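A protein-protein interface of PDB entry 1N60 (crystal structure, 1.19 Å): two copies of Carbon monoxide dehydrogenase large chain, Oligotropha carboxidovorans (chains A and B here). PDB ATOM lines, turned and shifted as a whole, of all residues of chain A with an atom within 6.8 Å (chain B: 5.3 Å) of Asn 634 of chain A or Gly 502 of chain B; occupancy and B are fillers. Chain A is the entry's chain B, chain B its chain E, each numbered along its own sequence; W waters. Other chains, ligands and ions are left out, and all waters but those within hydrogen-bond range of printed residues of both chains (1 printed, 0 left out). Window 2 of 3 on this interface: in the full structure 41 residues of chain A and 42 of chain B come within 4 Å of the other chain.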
ATOM      1  N   MET A 598     -40.090 -22.360 -12.979  1.00  0.00           N
ATOM      2  CA  MET A 598     -39.069 -22.248 -13.996  1.00  0.00           C
ATOM      3  C   MET A 598     -39.559 -21.500 -15.198  1.00  0.00           C
ATOM      4  O   MET A 598     -38.800 -20.711 -15.777  1.00  0.00           O
ATOM      5  CB  MET A 598     -38.600 -23.609 -14.421  1.00  0.00           C
ATOM      6  CG  MET A 598     -37.966 -24.443 -13.372  1.00  0.00           C
ATOM      7  SD  MET A 598     -37.354 -26.035 -13.950  1.00  0.00           S
ATOM      8  CE  MET A 598     -35.905 -25.547 -14.717  1.00  0.00           C
ATOM      9  N   ALA A 629     -37.011 -33.127 -12.817  1.00  0.00           N
ATOM     10  CA  ALA A 629     -36.339 -33.926 -11.845  1.00  0.00           C
ATOM     11  C   ALA A 629     -34.980 -33.328 -11.547  1.00  0.00           C
ATOM     12  O   ALA A 629     -34.587 -33.182 -10.382  1.00  0.00           O
ATOM     13  CB  ALA A 629     -36.225 -35.331 -12.353  1.00  0.00           C
ATOM     14  N   TRP A 630     -34.231 -32.952 -12.585  1.00  0.00           N
ATOM     15  CA  TRP A 630     -32.938 -32.351 -12.316  1.00  0.00           C
ATOM     16  C   TRP A 630     -33.119 -31.060 -11.573  1.00  0.00           C
ATOM     17  O   TRP A 630     -32.426 -30.785 -10.601  1.00  0.00           O
ATOM     18  CB  TRP A 630     -32.213 -32.091 -13.635  1.00  0.00           C
ATOM     19  CG  TRP A 630     -30.931 -31.355 -13.477  1.00  0.00           C
ATOM     20  CD1 TRP A 630     -30.684 -30.104 -13.927  1.00  0.00           C
ATOM     21  CD2 TRP A 630     -29.795 -31.751 -12.741  1.00  0.00           C
ATOM     22  NE1 TRP A 630     -29.434 -29.697 -13.555  1.00  0.00           N
ATOM     23  CE2 TRP A 630     -28.851 -30.689 -12.824  1.00  0.00           C
ATOM     24  CE3 TRP A 630     -29.428 -32.892 -12.032  1.00  0.00           C
ATOM     25  CZ2 TRP A 630     -27.603 -30.764 -12.263  1.00  0.00           C
ATOM     26  CZ3 TRP A 630     -28.191 -32.936 -11.467  1.00  0.00           C
ATOM     27  CH2 TRP A 630     -27.297 -31.899 -11.597  1.00  0.00           C
ATOM     28  N   ALA A 631     -34.077 -30.247 -11.984  1.00  0.00           N
ATOM     29  CA  ALA A 631     -34.306 -28.993 -11.334  1.00  0.00           C
ATOM     30  C   ALA A 631     -34.625 -29.147  -9.854  1.00  0.00           C
ATOM     31  O   ALA A 631     -34.223 -28.328  -9.041  1.00  0.00           O
ATOM     32  CB  ALA A 631     -35.408 -28.222 -12.038  1.00  0.00           C
ATOM     33  N   SER A 632     -35.347 -30.199  -9.500  1.00  0.00           N
ATOM     34  CA  SER A 632     -35.711 -30.373  -8.101  1.00  0.00           C
ATOM     35  C   SER A 632     -34.493 -30.538  -7.202  1.00  0.00           C
ATOM     36  O   SER A 632     -34.569 -30.301  -6.013  1.00  0.00           O
ATOM     37  CB  SER A 632     -36.658 -31.592  -7.970  1.00  0.00           C
ATOM     38  OG  SER A 632     -35.926 -32.795  -8.008  1.00  0.00           O
ATOM     39  N   TYR A 633     -33.404 -30.995  -7.781  1.00  0.00           N
ATOM     40  CA  TYR A 633     -32.137 -31.139  -7.055  1.00  0.00           C
ATOM     41  C   TYR A 633     -31.206 -29.953  -7.269  1.00  0.00           C
ATOM     42  O   TYR A 633     -30.429 -29.597  -6.377  1.00  0.00           O
ATOM     43  CB  TYR A 633     -31.422 -32.402  -7.498  1.00  0.00           C
ATOM     44  CG  TYR A 633     -32.063 -33.690  -7.089  1.00  0.00           C
ATOM     45  CD1 TYR A 633     -33.007 -34.300  -7.858  1.00  0.00           C
ATOM     46  CD2 TYR A 633     -31.671 -34.347  -5.922  1.00  0.00           C
ATOM     47  CE1 TYR A 633     -33.559 -35.480  -7.527  1.00  0.00           C
ATOM     48  CE2 TYR A 633     -32.247 -35.538  -5.553  1.00  0.00           C
ATOM     49  CZ  TYR A 633     -33.202 -36.089  -6.384  1.00  0.00           C
ATOM     50  OH  TYR A 633     -33.683 -37.328  -6.021  1.00  0.00           O
ATOM     51  N   ASN A 634     -31.234 -29.367  -8.454  1.00  0.00           N
ATOM     52  CA  ASN A 634     -30.276 -28.357  -8.885  1.00  0.00           C
ATOM     53  C   ASN A 634     -30.721 -26.985  -8.561  1.00  0.00           C
ATOM     54  O   ASN A 634     -29.861 -26.131  -8.287  1.00  0.00           O
ATOM     55  CB  ASN A 634     -30.117 -28.483 -10.404  1.00  0.00           C
ATOM     56  CG  ASN A 634     -29.440 -27.290 -11.050  1.00  0.00           C
ATOM     57  OD1 ASN A 634     -30.101 -26.471 -11.708  1.00  0.00           O
ATOM     58  ND2 ASN A 634     -28.144 -27.199 -10.923  1.00  0.00           N
ATOM     59  N   SER A 635     -32.029 -26.727  -8.675  1.00  0.00           N
ATOM     60  CA  SER A 635     -32.515 -25.381  -8.421  1.00  0.00           C
ATOM     61  C   SER A 635     -33.882 -25.496  -7.807  1.00  0.00           C
ATOM     62  O   SER A 635     -34.911 -25.128  -8.381  1.00  0.00           O
ATOM     63  N   PRO A 636     -33.942 -26.035  -6.601  1.00  0.00           N
ATOM     64  CA  PRO A 636     -35.257 -26.178  -5.965  1.00  0.00           C
ATOM     65  C   PRO A 636     -35.924 -24.829  -5.821  1.00  0.00           C
ATOM     66  O   PRO A 636     -35.267 -23.895  -5.413  1.00  0.00           O
ATOM     67  CB  PRO A 636     -34.891 -26.753  -4.597  1.00  0.00           C
ATOM     68  CG  PRO A 636     -33.454 -26.412  -4.481  1.00  0.00           C
ATOM     69  CD  PRO A 636     -32.849 -26.579  -5.786  1.00  0.00           C
ATOM     70  N   PRO A 642     -36.069 -29.748  -1.778  1.00  0.00           N
ATOM     71  CA  PRO A 642     -35.366 -30.381  -2.892  1.00  0.00           C
ATOM     72  C   PRO A 642     -35.864 -31.794  -3.066  1.00  0.00           C
ATOM     73  O   PRO A 642     -36.489 -32.370  -2.179  1.00  0.00           O
ATOM     74  CB  PRO A 642     -33.908 -30.377  -2.421  1.00  0.00           C
ATOM     75  CG  PRO A 642     -33.830 -29.290  -1.444  1.00  0.00           C
ATOM     76  CD  PRO A 642     -35.170 -29.278  -0.742  1.00  0.00           C
ATOM     77  N   GLY A 643     -35.514 -32.352  -4.197  1.00  0.00           N
ATOM     78  CA  GLY A 643     -35.830 -33.716  -4.541  1.00  0.00           C
ATOM     79  C   GLY A 643     -37.217 -33.854  -5.136  1.00  0.00           C
ATOM     80  O   GLY A 643     -37.960 -32.912  -5.235  1.00  0.00           O
ATOM     81  N   SER B 349     -19.331 -25.850  -5.996  1.00  0.00           N
ATOM     82  CA  SER B 349     -18.830 -25.509  -7.305  1.00  0.00           C
ATOM     83  C   SER B 349     -18.502 -24.057  -7.503  1.00  0.00           C
ATOM     84  O   SER B 349     -17.690 -23.729  -8.330  1.00  0.00           O
ATOM     85  CB  SER B 349     -19.796 -25.973  -8.402  1.00  0.00           C
ATOM     86  OG  SER B 349     -20.881 -25.124  -8.514  1.00  0.00           O
ATOM     87  N   ASP B 499     -23.577 -25.923  -4.054  1.00  0.00           N
ATOM     88  CA  ASP B 499     -23.928 -27.078  -4.834  1.00  0.00           C
ATOM     89  C   ASP B 499     -22.657 -27.877  -5.091  1.00  0.00           C
ATOM     90  O   ASP B 499     -21.583 -27.338  -5.178  1.00  0.00           O
ATOM     91  CB  ASP B 499     -24.591 -26.674  -6.156  1.00  0.00           C
ATOM     92  CG  ASP B 499     -23.621 -26.007  -7.069  1.00  0.00           C
ATOM     93  OD1 ASP B 499     -23.539 -24.768  -6.964  1.00  0.00           O
ATOM     94  OD2 ASP B 499     -22.988 -26.650  -7.909  1.00  0.00           O
ATOM     95  N   ILE B 500     -22.831 -29.162  -5.231  1.00  0.00           N
ATOM     96  CA  ILE B 500     -21.773 -30.074  -5.653  1.00  0.00           C
ATOM     97  C   ILE B 500     -22.138 -30.483  -7.044  1.00  0.00           C
ATOM     98  O   ILE B 500     -23.133 -31.169  -7.285  1.00  0.00           O
ATOM     99  CB  ILE B 500     -21.669 -31.311  -4.766  1.00  0.00           C
ATOM    100  CG1 ILE B 500     -21.269 -30.907  -3.356  1.00  0.00           C
ATOM    101  CG2 ILE B 500     -20.711 -32.287  -5.358  1.00  0.00           C
ATOM    102  CD1 ILE B 500     -19.809 -30.360  -3.212  1.00  0.00           C
ATOM    103  N   LEU B 501     -21.347 -29.996  -7.975  1.00  0.00           N
ATOM    104  CA  LEU B 501     -21.561 -30.242  -9.389  1.00  0.00           C
ATOM    105  C   LEU B 501     -23.030 -30.107  -9.790  1.00  0.00           C
ATOM    106  O   LEU B 501     -23.586 -30.917 -10.551  1.00  0.00           O
ATOM    107  CB  LEU B 501     -21.044 -31.580  -9.807  1.00  0.00           C
ATOM    108  CG  LEU B 501     -19.501 -31.671  -9.691  1.00  0.00           C
ATOM    109  CD1 LEU B 501     -18.972 -32.953 -10.171  1.00  0.00           C
ATOM    110  CD2 LEU B 501     -18.726 -30.603 -10.403  1.00  0.00           C
ATOM    111  N   GLY B 502     -23.627 -29.028  -9.321  1.00  0.00           N
ATOM    112  CA  GLY B 502     -24.975 -28.702  -9.676  1.00  0.00           C
ATOM    113  C   GLY B 502     -26.075 -29.260  -8.797  1.00  0.00           C
ATOM    114  O   GLY B 502     -27.215 -28.904  -8.979  1.00  0.00           O
ATOM    115  N   VAL B 503     -25.751 -30.145  -7.882  1.00  0.00           N
ATOM    116  CA  VAL B 503     -26.723 -30.655  -6.937  1.00  0.00           C
ATOM    117  C   VAL B 503     -26.656 -29.792  -5.699  1.00  0.00           C
ATOM    118  O   VAL B 503     -25.608 -29.682  -5.055  1.00  0.00           O
ATOM    119  CB  VAL B 503     -26.486 -32.119  -6.600  1.00  0.00           C
ATOM    120  CG1 VAL B 503     -27.487 -32.514  -5.617  1.00  0.00           C
ATOM    121  CG2 VAL B 503     -26.515 -32.951  -7.845  1.00  0.00           C
ATOM    122  N   SER B 504     -27.735 -29.110  -5.387  1.00  0.00           N
ATOM    123  CA  SER B 504     -27.761 -28.276  -4.212  1.00  0.00           C
ATOM    124  C   SER B 504     -27.433 -29.033  -2.964  1.00  0.00           C
ATOM    125  O   SER B 504     -27.740 -30.204  -2.816  1.00  0.00           O
ATOM    126  CB  SER B 504     -29.172 -27.670  -4.115  1.00  0.00           C
ATOM    127  OG  SER B 504     -29.196 -26.580  -3.217  1.00  0.00           O
HETATM  128  O   HOH W   1     -27.122 -25.674  -8.057  1.00  0.00           O
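Of the printed residues of chain B, Asn 634 of chain A touches Gly 502.
Of the printed residues of chain A, Leu 501 of chain B touches Trp 630 (3.98 Å).
Gly 502 of chain B touches just these residues of chain A: Trp 630 and Asn 634.
Of the printed residues of chain A, Val 503 of chain B touches Trp 630 and Tyr 633.
Printed residues of chain A within 4 Å of Ser 504 of chain B: Tyr 633 (2.9 Å).
The nearest residue of chain A that does not touch Gly 502 of chain B is Tyr 633 of chain A (4.2 Å).
No position is printed for both chains.
Of the 6 pairs that touch across the chains among the printed residues, none has its exchanged pair printed and touching as well.
Hydrophobic or aromatic side chains of chain A within 4 Å of the printed part of chain B: Trp 630.
Of the 7 printed residues of chain B, 4 touch a printed residue of chain A.
Hydrophobic or aromatic side chains of chain B within 4 Å of the printed part of chain A: Val 503.
Water W1 lies within hydrogen-bond range of the backbone carbonyl oxygen of Asn 634 of chain A (2.8 Å) and the backbone carbonyl oxygen of Gly 502 of chain B (3.4 Å).
The side-chain carboxylate (OD2) of Asp 499 of chain B lies within hydrogen-bond range of the backbone NH (N) of Gly 502 of chain B.
Among the printed residues, merely in contact across the chains: Trp 630 of chain A with Gly 502 of chain B (3.8 Å), Tyr 633 of chain A with Val 503 of chain B (3.8 Å), Trp 630 of chain A with Val 503 of chain B (3.97 Å) and Trp 630 of chain A with Leu 501 of chain B (3.98 Å).
The backbone carbonyl oxygen (O) of Tyr 633 of chain A lies within hydrogen-bond range of the backbone NH (N) of Ser 504 of chain B (2.9 Å).
ND2 of Asn 634 of chain A is in hydrogen-bond range of O of Gly 502 of chain B.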
